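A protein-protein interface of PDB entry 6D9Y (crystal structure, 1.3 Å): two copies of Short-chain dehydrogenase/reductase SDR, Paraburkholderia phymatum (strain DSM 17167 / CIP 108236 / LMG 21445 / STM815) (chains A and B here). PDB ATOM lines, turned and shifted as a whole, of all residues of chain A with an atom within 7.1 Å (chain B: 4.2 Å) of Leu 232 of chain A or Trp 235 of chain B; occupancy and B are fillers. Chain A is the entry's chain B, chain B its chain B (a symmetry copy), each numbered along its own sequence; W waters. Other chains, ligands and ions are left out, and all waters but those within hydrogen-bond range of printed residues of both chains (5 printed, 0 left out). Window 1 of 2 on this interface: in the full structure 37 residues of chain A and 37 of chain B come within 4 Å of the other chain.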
ATOM      1  N   ASN A  10     -23.681  -4.755  10.293  1.00  0.00           N
ATOM      2  CA  ASN A  10     -24.304  -6.050  10.121  1.00  0.00           C
ATOM      3  C   ASN A  10     -24.676  -6.628  11.478  1.00  0.00           C
ATOM      4  O   ASN A  10     -23.966  -6.450  12.474  1.00  0.00           O
ATOM      5  CB  ASN A  10     -23.320  -6.977   9.422  1.00  0.00           C
ATOM      6  CG  ASN A  10     -22.936  -6.476   8.022  1.00  0.00           C
ATOM      7  OD1 ASN A  10     -23.649  -5.714   7.372  1.00  0.00           O
ATOM      8  ND2 ASN A  10     -21.785  -6.944   7.560  1.00  0.00           N
ATOM      9  N   ILE A  12     -24.534  -9.661  13.401  1.00  0.00           N
ATOM     10  CA  ILE A  12     -23.939 -10.987  13.490  1.00  0.00           C
ATOM     11  C   ILE A  12     -24.785 -11.807  14.448  1.00  0.00           C
ATOM     12  O   ILE A  12     -25.141 -11.345  15.544  1.00  0.00           O
ATOM     13  CB  ILE A  12     -22.493 -10.874  13.996  1.00  0.00           C
ATOM     14  CG1 ILE A  12     -21.677  -9.936  13.087  1.00  0.00           C
ATOM     15  CG2 ILE A  12     -21.825 -12.262  14.088  1.00  0.00           C
ATOM     16  CD1 ILE A  12     -20.270  -9.654  13.642  1.00  0.00           C
ATOM     17  N   ARG A  35     -18.983  -6.083  20.787  1.00  0.00           N
ATOM     18  CA  ARG A  35     -19.736  -6.516  19.617  1.00  0.00           C
ATOM     19  C   ARG A  35     -20.345  -7.889  19.837  1.00  0.00           C
ATOM     20  O   ARG A  35     -21.485  -8.136  19.426  1.00  0.00           O
ATOM     21  CB  ARG A  35     -18.851  -6.489  18.363  1.00  0.00           C
ATOM     22  CG  ARG A  35     -19.561  -6.875  17.053  1.00  0.00           C
ATOM     23  CD  ARG A  35     -20.621  -5.845  16.664  1.00  0.00           C
ATOM     24  NE  ARG A  35     -21.189  -6.111  15.341  1.00  0.00           N
ATOM     25  CZ  ARG A  35     -20.632  -5.730  14.201  1.00  0.00           C
ATOM     26  NH1 ARG A  35     -19.471  -5.070  14.216  1.00  0.00           N
ATOM     27  NH2 ARG A  35     -21.243  -5.991  13.055  1.00  0.00           N
ATOM     28  N   VAL A 148     -10.558 -18.000  16.345  1.00  0.00           N
ATOM     29  CA  VAL A 148     -10.014 -16.866  15.594  1.00  0.00           C
ATOM     30  C   VAL A 148      -8.756 -16.419  16.329  1.00  0.00           C
ATOM     31  O   VAL A 148      -8.826 -15.989  17.500  1.00  0.00           O
ATOM     32  CB  VAL A 148     -11.014 -15.702  15.474  1.00  0.00           C
ATOM     33  CG1 VAL A 148     -10.479 -14.698  14.474  1.00  0.00           C
ATOM     34  CG2 VAL A 148     -12.407 -16.190  15.043  1.00  0.00           C
ATOM     35  N   ALA A 192      -7.076 -17.042  11.182  1.00  0.00           N
ATOM     36  CA  ALA A 192      -6.313 -15.956  11.782  1.00  0.00           C
ATOM     37  C   ALA A 192      -6.675 -14.651  11.097  1.00  0.00           C
ATOM     38  O   ALA A 192      -7.139 -14.629   9.951  1.00  0.00           O
ATOM     39  CB  ALA A 192      -4.800 -16.199  11.619  1.00  0.00           C
ATOM     40  N   VAL A 193      -6.424 -13.544  11.799  1.00  0.00           N
ATOM     41  CA  VAL A 193      -6.531 -12.204  11.214  1.00  0.00           C
ATOM     42  C   VAL A 193      -5.190 -11.513  11.354  1.00  0.00           C
ATOM     43  O   VAL A 193      -4.435 -11.735  12.309  1.00  0.00           O
ATOM     44  CB  VAL A 193      -7.647 -11.270  11.765  1.00  0.00           C
ATOM     45  CG1 VAL A 193      -9.027 -11.798  11.414  1.00  0.00           C
ATOM     46  CG2 VAL A 193      -7.488 -11.039  13.275  1.00  0.00           C
ATOM     47  N   THR A 194      -4.893 -10.640  10.384  1.00  0.00           N
ATOM     48  CA  THR A 194      -3.630  -9.881  10.388  1.00  0.00           C
ATOM     49  C   THR A 194      -3.895  -8.381  10.402  1.00  0.00           C
ATOM     50  O   THR A 194      -3.882  -7.722   9.347  1.00  0.00           O
ATOM     51  CB  THR A 194      -2.701 -10.294   9.237  1.00  0.00           C
ATOM     52  OG1 THR A 194      -3.416 -10.279   7.988  1.00  0.00           O
ATOM     53  CG2 THR A 194      -2.172 -11.690   9.451  1.00  0.00           C
ATOM     54  N   ASP A 227     -13.203  -1.295  16.706  1.00  0.00           N
ATOM     55  CA  ASP A 227     -14.543  -1.739  16.299  1.00  0.00           C
ATOM     56  C   ASP A 227     -14.555  -2.347  14.908  1.00  0.00           C
ATOM     57  O   ASP A 227     -15.304  -3.302  14.652  1.00  0.00           O
ATOM     58  CB  ASP A 227     -15.534  -0.579  16.354  1.00  0.00           C
ATOM     59  CG  ASP A 227     -15.876  -0.156  17.760  1.00  0.00           C
ATOM     60  OD1 ASP A 227     -15.715  -0.941  18.711  1.00  0.00           O
ATOM     61  OD2 ASP A 227     -16.321   1.010  17.918  1.00  0.00           O
ATOM     62  N   GLU A 228     -13.767  -1.803  13.976  1.00  0.00           N
ATOM     63  CA  GLU A 228     -13.655  -2.380  12.633  1.00  0.00           C
ATOM     64  C   GLU A 228     -13.044  -3.770  12.691  1.00  0.00           C
ATOM     65  O   GLU A 228     -13.451  -4.684  11.965  1.00  0.00           O
ATOM     66  CB  GLU A 228     -12.771  -1.481  11.759  1.00  0.00           C
ATOM     67  CG  GLU A 228     -13.398  -0.113  11.477  1.00  0.00           C
ATOM     68  CD  GLU A 228     -12.459   0.868  10.805  1.00  0.00           C
ATOM     69  OE1 GLU A 228     -11.229   0.783  11.012  1.00  0.00           O
ATOM     70  OE2 GLU A 228     -12.965   1.729  10.057  1.00  0.00           O
ATOM     71  N   ALA A 229     -12.028  -3.935  13.544  1.00  0.00           N
ATOM     72  CA  ALA A 229     -11.435  -5.257  13.701  1.00  0.00           C
ATOM     73  C   ALA A 229     -12.466  -6.261  14.206  1.00  0.00           C
ATOM     74  O   ALA A 229     -12.555  -7.388  13.694  1.00  0.00           O
ATOM     75  CB  ALA A 229     -10.240  -5.186  14.641  1.00  0.00           C
ATOM     76  N   ALA A 230     -13.287  -5.844  15.182  1.00  0.00           N
ATOM     77  CA  ALA A 230     -14.293  -6.735  15.765  1.00  0.00           C
ATOM     78  C   ALA A 230     -15.298  -7.207  14.729  1.00  0.00           C
ATOM     79  O   ALA A 230     -15.766  -8.355  14.801  1.00  0.00           O
ATOM     80  CB  ALA A 230     -14.991  -6.034  16.935  1.00  0.00           C
ATOM     81  N   SER A 231     -15.629  -6.367  13.747  1.00  0.00           N
ATOM     82  CA  SER A 231     -16.592  -6.794  12.725  1.00  0.00           C
ATOM     83  C   SER A 231     -16.119  -8.045  12.003  1.00  0.00           C
ATOM     84  O   SER A 231     -16.901  -8.976  11.769  1.00  0.00           O
ATOM     85  CB  SER A 231     -16.819  -5.692  11.693  1.00  0.00           C
ATOM     86  OG  SER A 231     -17.430  -4.566  12.289  1.00  0.00           O
ATOM     87  N   LEU A 232     -14.848  -8.071  11.592  1.00  0.00           N
ATOM     88  CA  LEU A 232     -14.344  -9.216  10.861  1.00  0.00           C
ATOM     89  C   LEU A 232     -14.036 -10.379  11.799  1.00  0.00           C
ATOM     90  O   LEU A 232     -14.316 -11.541  11.466  1.00  0.00           O
ATOM     91  CB  LEU A 232     -13.114  -8.807  10.060  1.00  0.00           C
ATOM     92  CG  LEU A 232     -12.412  -9.931   9.290  1.00  0.00           C
ATOM     93  CD1 LEU A 232     -13.312 -10.726   8.377  1.00  0.00           C
ATOM     94  CD2 LEU A 232     -11.226  -9.336   8.513  1.00  0.00           C
ATOM     95  N   ILE A 233     -13.459 -10.097  12.969  1.00  0.00           N
ATOM     96  CA  ILE A 233     -13.137 -11.161  13.915  1.00  0.00           C
ATOM     97  C   ILE A 233     -14.381 -11.957  14.274  1.00  0.00           C
ATOM     98  O   ILE A 233     -14.356 -13.199  14.293  1.00  0.00           O
ATOM     99  CB  ILE A 233     -12.468 -10.558  15.160  1.00  0.00           C
ATOM    100  CG1 ILE A 233     -11.059 -10.023  14.803  1.00  0.00           C
ATOM    101  CG2 ILE A 233     -12.417 -11.577  16.315  1.00  0.00           C
ATOM    102  CD1 ILE A 233     -10.474  -9.106  15.866  1.00  0.00           C
ATOM    103  N   LEU A 234     -15.501 -11.271  14.534  1.00  0.00           N
ATOM    104  CA  LEU A 234     -16.691 -12.013  14.913  1.00  0.00           C
ATOM    105  C   LEU A 234     -17.424 -12.611  13.727  1.00  0.00           C
ATOM    106  O   LEU A 234     -18.173 -13.575  13.925  1.00  0.00           O
ATOM    107  CB  LEU A 234     -17.600 -11.165  15.804  1.00  0.00           C
ATOM    108  CG  LEU A 234     -16.978 -10.931  17.182  1.00  0.00           C
ATOM    109  CD1 LEU A 234     -17.825  -9.928  17.951  1.00  0.00           C
ATOM    110  CD2 LEU A 234     -16.837 -12.227  17.991  1.00  0.00           C
ATOM    111  N   TRP A 235     -17.225 -12.097  12.510  1.00  0.00           N
ATOM    112  CA  TRP A 235     -17.694 -12.823  11.330  1.00  0.00           C
ATOM    113  C   TRP A 235     -17.068 -14.211  11.302  1.00  0.00           C
ATOM    114  O   TRP A 235     -17.752 -15.226  11.093  1.00  0.00           O
ATOM    115  CB  TRP A 235     -17.397 -12.036  10.038  1.00  0.00           C
ATOM    116  CG  TRP A 235     -18.034 -12.709   8.829  1.00  0.00           C
ATOM    117  CD1 TRP A 235     -19.307 -12.514   8.378  1.00  0.00           C
ATOM    118  CD2 TRP A 235     -17.465 -13.751   8.006  1.00  0.00           C
ATOM    119  NE1 TRP A 235     -19.559 -13.346   7.306  1.00  0.00           N
ATOM    120  CE2 TRP A 235     -18.452 -14.120   7.070  1.00  0.00           C
ATOM    121  CE3 TRP A 235     -16.221 -14.412   7.975  1.00  0.00           C
ATOM    122  CZ2 TRP A 235     -18.227 -15.117   6.095  1.00  0.00           C
ATOM    123  CZ3 TRP A 235     -15.993 -15.391   6.992  1.00  0.00           C
ATOM    124  CH2 TRP A 235     -17.005 -15.741   6.074  1.00  0.00           C
ATOM    125  N   LEU A 236     -15.747 -14.278  11.536  1.00  0.00           N
ATOM    126  CA  LEU A 236     -15.023 -15.549  11.571  1.00  0.00           C
ATOM    127  C   LEU A 236     -15.437 -16.414  12.760  1.00  0.00           C
ATOM    128  O   LEU A 236     -15.199 -17.633  12.750  1.00  0.00           O
ATOM    129  CB  LEU A 236     -13.510 -15.248  11.608  1.00  0.00           C
ATOM    130  CG  LEU A 236     -12.969 -14.580  10.328  1.00  0.00           C
ATOM    131  CD1 LEU A 236     -11.578 -14.031  10.594  1.00  0.00           C
ATOM    132  CD2 LEU A 236     -12.940 -15.593   9.208  1.00  0.00           C
ATOM    133  N   GLY A 237     -16.029 -15.815  13.789  1.00  0.00           N
ATOM    134  CA  GLY A 237     -16.553 -16.544  14.913  1.00  0.00           C
ATOM    135  C   GLY A 237     -18.005 -16.930  14.774  1.00  0.00           C
ATOM    136  O   GLY A 237     -18.580 -17.428  15.751  1.00  0.00           O
ATOM    137  N   SER A 238     -18.601 -16.746  13.589  1.00  0.00           N
ATOM    138  CA  SER A 238     -20.026 -16.988  13.379  1.00  0.00           C
ATOM    139  C   SER A 238     -20.222 -18.181  12.451  1.00  0.00           C
ATOM    140  O   SER A 238     -19.315 -18.608  11.729  1.00  0.00           O
ATOM    141  CB  SER A 238     -20.718 -15.732  12.807  1.00  0.00           C
ATOM    142  OG  SER A 238     -20.484 -15.571  11.405  1.00  0.00           O
ATOM    143  N   PHE A 249      -7.164 -13.778   7.277  1.00  0.00           N
ATOM    144  CA  PHE A 249      -8.034 -12.689   6.837  1.00  0.00           C
ATOM    145  C   PHE A 249      -7.385 -11.367   7.206  1.00  0.00           C
ATOM    146  O   PHE A 249      -7.026 -11.141   8.361  1.00  0.00           O
ATOM    147  CB  PHE A 249      -9.404 -12.828   7.499  1.00  0.00           C
ATOM    148  CG  PHE A 249     -10.199 -13.986   6.953  1.00  0.00           C
ATOM    149  CD1 PHE A 249      -9.868 -15.319   7.286  1.00  0.00           C
ATOM    150  CD2 PHE A 249     -11.277 -13.740   6.129  1.00  0.00           C
ATOM    151  CE1 PHE A 249     -10.605 -16.377   6.739  1.00  0.00           C
ATOM    152  CE2 PHE A 249     -12.043 -14.801   5.590  1.00  0.00           C
ATOM    153  CZ  PHE A 249     -11.689 -16.120   5.888  1.00  0.00           C
ATOM    154  N   ASP A 250      -7.221 -10.500   6.218  1.00  0.00           N
ATOM    155  CA  ASP A 250      -6.384  -9.316   6.400  1.00  0.00           C
ATOM    156  C   ASP A 250      -7.138  -8.108   6.948  1.00  0.00           C
ATOM    157  O   ASP A 250      -8.265  -7.827   6.522  1.00  0.00           O
ATOM    158  CB  ASP A 250      -5.710  -8.933   5.083  1.00  0.00           C
ATOM    159  CG  ASP A 250      -4.601  -7.956   5.306  1.00  0.00           C
ATOM    160  OD1 ASP A 250      -3.534  -8.355   5.844  1.00  0.00           O
ATOM    161  OD2 ASP A 250      -4.822  -6.754   5.014  1.00  0.00           O
ATOM    162  N   LEU A 251      -6.457  -7.339   7.808  1.00  0.00           N
ATOM    163  CA  LEU A 251      -6.953  -6.083   8.392  1.00  0.00           C
ATOM    164  C   LEU A 251      -5.870  -5.011   8.371  1.00  0.00           C
ATOM    165  O   LEU A 251      -5.658  -4.292   9.347  1.00  0.00           O
ATOM    166  CB  LEU A 251      -7.458  -6.280   9.830  1.00  0.00           C
ATOM    167  CG  LEU A 251      -8.855  -6.882   9.998  1.00  0.00           C
ATOM    168  CD1 LEU A 251      -9.092  -7.142  11.477  1.00  0.00           C
ATOM    169  CD2 LEU A 251      -9.927  -5.928   9.477  1.00  0.00           C
ATOM    170  N   ILE B  12     -26.846  -9.165   6.954  1.00  0.00           N
ATOM    171  CA  ILE B  12     -25.988  -8.175   6.318  1.00  0.00           C
ATOM    172  C   ILE B  12     -26.842  -6.961   6.001  1.00  0.00           C
ATOM    173  O   ILE B  12     -27.952  -7.084   5.456  1.00  0.00           O
ATOM    174  CB  ILE B  12     -25.377  -8.765   5.037  1.00  0.00           C
ATOM    175  CG1 ILE B  12     -24.619 -10.068   5.355  1.00  0.00           C
ATOM    176  CG2 ILE B  12     -24.448  -7.747   4.345  1.00  0.00           C
ATOM    177  CD1 ILE B  12     -24.131 -10.789   4.086  1.00  0.00           C
ATOM    178  N   SER B 231     -22.347 -15.565   1.562  1.00  0.00           N
ATOM    179  CA  SER B 231     -22.187 -14.951   2.886  1.00  0.00           C
ATOM    180  C   SER B 231     -20.928 -14.102   2.956  1.00  0.00           C
ATOM    181  O   SER B 231     -20.946 -12.985   3.491  1.00  0.00           O
ATOM    182  CB  SER B 231     -22.115 -16.017   3.977  1.00  0.00           C
ATOM    183  OG  SER B 231     -23.339 -16.718   4.072  1.00  0.00           O
ATOM    184  N   LEU B 232     -19.804 -14.631   2.466  1.00  0.00           N
ATOM    185  CA  LEU B 232     -18.560 -13.890   2.538  1.00  0.00           C
ATOM    186  C   LEU B 232     -18.493 -12.814   1.459  1.00  0.00           C
ATOM    187  O   LEU B 232     -18.021 -11.697   1.720  1.00  0.00           O
ATOM    188  CB  LEU B 232     -17.386 -14.856   2.435  1.00  0.00           C
ATOM    189  CG  LEU B 232     -15.993 -14.218   2.416  1.00  0.00           C
ATOM    190  CD1 LEU B 232     -15.716 -13.279   3.563  1.00  0.00           C
ATOM    191  CD2 LEU B 232     -14.936 -15.333   2.348  1.00  0.00           C
ATOM    192  N   ILE B 233     -18.951 -13.124   0.245  1.00  0.00           N
ATOM    193  CA  ILE B 233     -18.917 -12.142  -0.835  1.00  0.00           C
ATOM    194  C   ILE B 233     -19.672 -10.883  -0.441  1.00  0.00           C
ATOM    195  O   ILE B 233     -19.186  -9.760  -0.653  1.00  0.00           O
ATOM    196  CB  ILE B 233     -19.485 -12.768  -2.118  1.00  0.00           C
ATOM    197  CG1 ILE B 233     -18.519 -13.853  -2.656  1.00  0.00           C
ATOM    198  CG2 ILE B 233     -19.783 -11.692  -3.180  1.00  0.00           C
ATOM    199  CD1 ILE B 233     -19.151 -14.760  -3.701  1.00  0.00           C
ATOM    200  N   LEU B 234     -20.855 -11.035   0.166  1.00  0.00           N
ATOM    201  CA  LEU B 234     -21.608  -9.844   0.517  1.00  0.00           C
ATOM    202  C   LEU B 234     -21.123  -9.188   1.797  1.00  0.00           C
ATOM    203  O   LEU B 234     -21.378  -7.991   1.977  1.00  0.00           O
ATOM    204  CB  LEU B 234     -23.109 -10.133   0.534  1.00  0.00           C
ATOM    205  CG  LEU B 234     -23.650 -10.386  -0.875  1.00  0.00           C
ATOM    206  CD1 LEU B 234     -25.093 -10.858  -0.781  1.00  0.00           C
ATOM    207  CD2 LEU B 234     -23.561  -9.143  -1.770  1.00  0.00           C
ATOM    208  N   TRP B 235     -20.422  -9.910   2.675  1.00  0.00           N
ATOM    209  CA  TRP B 235     -19.712  -9.240   3.765  1.00  0.00           C
ATOM    210  C   TRP B 235     -18.735  -8.223   3.189  1.00  0.00           C
ATOM    211  O   TRP B 235     -18.670  -7.065   3.631  1.00  0.00           O
ATOM    212  CB  TRP B 235     -19.003 -10.260   4.678  1.00  0.00           C
ATOM    213  CG  TRP B 235     -18.410  -9.577   5.903  1.00  0.00           C
ATOM    214  CD1 TRP B 235     -19.058  -9.327   7.078  1.00  0.00           C
ATOM    215  CD2 TRP B 235     -17.105  -8.969   6.021  1.00  0.00           C
ATOM    216  NE1 TRP B 235     -18.230  -8.629   7.933  1.00  0.00           N
ATOM    217  CE2 TRP B 235     -17.037  -8.388   7.303  1.00  0.00           C
ATOM    218  CE3 TRP B 235     -15.992  -8.855   5.165  1.00  0.00           C
ATOM    219  CZ2 TRP B 235     -15.884  -7.710   7.759  1.00  0.00           C
ATOM    220  CZ3 TRP B 235     -14.839  -8.195   5.628  1.00  0.00           C
ATOM    221  CH2 TRP B 235     -14.807  -7.618   6.915  1.00  0.00           C
ATOM    222  N   LEU B 236     -17.967  -8.640   2.169  1.00  0.00           N
ATOM    223  CA  LEU B 236     -17.009  -7.760   1.500  1.00  0.00           C
ATOM    224  C   LEU B 236     -17.702  -6.637   0.728  1.00  0.00           C
ATOM    225  O   LEU B 236     -17.063  -5.622   0.408  1.00  0.00           O
ATOM    226  CB  LEU B 236     -16.131  -8.614   0.563  1.00  0.00           C
ATOM    227  CG  LEU B 236     -15.219  -9.619   1.296  1.00  0.00           C
ATOM    228  CD1 LEU B 236     -14.663 -10.619   0.298  1.00  0.00           C
ATOM    229  CD2 LEU B 236     -14.102  -8.872   1.984  1.00  0.00           C
ATOM    230  N   GLY B 237     -18.981  -6.804   0.404  1.00  0.00           N
ATOM    231  CA  GLY B 237     -19.759  -5.772  -0.231  1.00  0.00           C
ATOM    232  C   GLY B 237     -20.499  -4.879   0.733  1.00  0.00           C
ATOM    233  O   GLY B 237     -21.308  -4.060   0.278  1.00  0.00           O
ATOM    234  N   SER B 238     -20.225  -4.988   2.040  1.00  0.00           N
ATOM    235  CA  SER B 238     -20.958  -4.246   3.063  1.00  0.00           C
ATOM    236  C   SER B 238     -20.042  -3.220   3.720  1.00  0.00           C
ATOM    237  O   SER B 238     -18.812  -3.288   3.637  1.00  0.00           O
ATOM    238  CB  SER B 238     -21.550  -5.205   4.118  1.00  0.00           C
ATOM    239  OG  SER B 238     -20.572  -5.647   5.064  1.00  0.00           O
ATOM    240  N   ASP B 240     -19.401  -3.040   6.828  1.00  0.00           N
ATOM    241  CA  ASP B 240     -18.578  -3.687   7.858  1.00  0.00           C
ATOM    242  C   ASP B 240     -17.177  -3.994   7.343  1.00  0.00           C
ATOM    243  O   ASP B 240     -16.230  -4.063   8.137  1.00  0.00           O
ATOM    244  CB  ASP B 240     -19.217  -5.000   8.355  1.00  0.00           C
ATOM    245  CG  ASP B 240     -20.276  -4.799   9.457  1.00  0.00           C
ATOM    246  OD1 ASP B 240     -21.253  -4.059   9.251  1.00  0.00           O
ATOM    247  OD2 ASP B 240     -20.148  -5.443  10.518  1.00  0.00           O
ATOM    248  N   CYS B 241     -17.027  -4.238   6.037  1.00  0.00           N
ATOM    249  CA  CYS B 241     -15.705  -4.366   5.425  1.00  0.00           C
ATOM    250  C   CYS B 241     -15.164  -2.955   5.323  1.00  0.00           C
ATOM    251  O   CYS B 241     -15.644  -2.156   4.514  1.00  0.00           O
ATOM    252  CB  CYS B 241     -15.816  -5.006   4.045  1.00  0.00           C
ATOM    253  SG  CYS B 241     -14.207  -5.177   3.242  1.00  0.00           S
HETATM  254  O   HOH W   1     -19.355  -8.128  10.467  1.00  0.00           O
HETATM  255  O   HOH W   2     -16.435  -2.665  10.589  1.00  0.00           O
HETATM  256  O   HOH W   3     -22.106 -12.996   6.154  1.00  0.00           O
HETATM  257  O   HOH W   4     -13.869  -5.254   9.274  1.00  0.00           O
HETATM  258  O   HOH W   5     -22.388  -3.232   7.023  1.00  0.00           O
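Of chain B, only Trp 235 (3.7 Å) comes within 4 Å of Leu 232 of chain A.
Of chain A, only Asn 10, Leu 232 and Trp 235 come within 4 Å of Trp 235 of chain B.
Printed residues of chain A within 4 Å of Leu 232 of chain B: Trp 235.
Of the printed residues of chain A, Asp 240 of chain B touches Asn 10, Arg 35 and Ser 231.
Ile 12 of chain B touches Asn 10 of chain A (CA to OD1, 3.6 Å).
Trp 235 of chain B touches Asn 10 of chain A (CD1 to ND2, 3.7 Å).
Trp 235 of chain B touches Leu 232 of chain A.
Leu 232 of chain B touches Trp 235 of chain A (CD1 to CH2, 3.7 Å).
Trp 235 of chain A touches Trp 235 of chain B (CD1 to CD1, 3.5 Å).
Of the 11 printed residues of chain B, 5 touch a printed residue of chain A.
Hydrophobic or aromatic side chains of chain B that line the printed part of chain A: Ile 12, Leu 232 and Trp 235.
Along chain B the printed residues that touch a printed residue of chain A span positions 12 to 240.
Among the printed residues, Asp or Glu carboxylates within 4 Å of a Lys or Arg side-chain nitrogen of the other chain: Arg 35 of chain A with Asp 240 of chain B (2.8 Å).
Leu 232 of chain A touches Trp 235 of chain B, and with the chains exchanged Trp 235 of chain A touches Leu 232 of chain B.
Trp 235 of chain B touches its own counterpart, Trp 235 of chain A.
9 positions are printed for both chains.
Of the 9 pairs that touch across the chains among the printed residues, 3 have their exchanged pair printed and touching as well.
NH2 of Arg 35 of chain A lies within hydrogen-bond range of O of Asn 10 of chain A, 2.8 Å away.
The side-chain hydroxyl (OG) of Ser 231 of chain A is in hydrogen-bond range of the guanidinium group (NH1) of Arg 35 of chain A.
O of Asp 227 of chain A lies within hydrogen-bond range of OG of Ser 231 of chain A, at 3.4 Å.
The backbone carbonyl oxygen of Trp 235 of chain A lies within hydrogen-bond range of the side-chain hydroxyl of Ser 238 of chain A (2.8 Å).
O of Trp 235 of chain B sits at hydrogen-bond distance from OG of Ser 238 of chain B, 2.8 Å away.
The side-chain hydroxyl (OG) of Ser 238 of chain B lies close to the backbone NH (N) of Asp 240 of chain B (3.4 Å).
ND2 of Asn 10 of chain A is in hydrogen-bond range of OG of Ser 238 of chain B, at 3.1 Å.
The backbone NH (N) of Asn 10 of chain A sits at hydrogen-bond distance from the side-chain carboxylate (OD1) of Asp 240 of chain B, at 2.7 Å.
The side-chain carboxylate of Asp 240 of chain B is in salt-bridge range of the guanidinium group of Arg 35 of chain A, at 2.8 Å.
The side-chain hydroxyl (OG) of Ser 231 of chain A sits at hydrogen-bond distance from the side-chain carboxylate (OD2) of Asp 240 of chain B (3.4 Å).
Water W5 bridges OD1 of Asp 240 of chain B (2.6 Å) and OD1 of Asn 10 of chain A (2.8 Å).
Water W2 bridges OG of Ser 231 of chain A and O of Asp 240 of chain B.
Water W4 bridges O of Glu 228 of chain A (2.8 Å) and O of Asp 240 of chain B (2.9 Å).
Water W1 lies within hydrogen-bond range of OD2 of Asp 240 of chain B (2.8 Å), NE1 of Trp 235 of chain B (2.8 Å) and O of Ser 231 of chain A (2.9 Å).
Water W3 bridges NE1 of Trp 235 of chain A (2.8 Å) and O of Ser 231 of chain B (2.9 Å).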
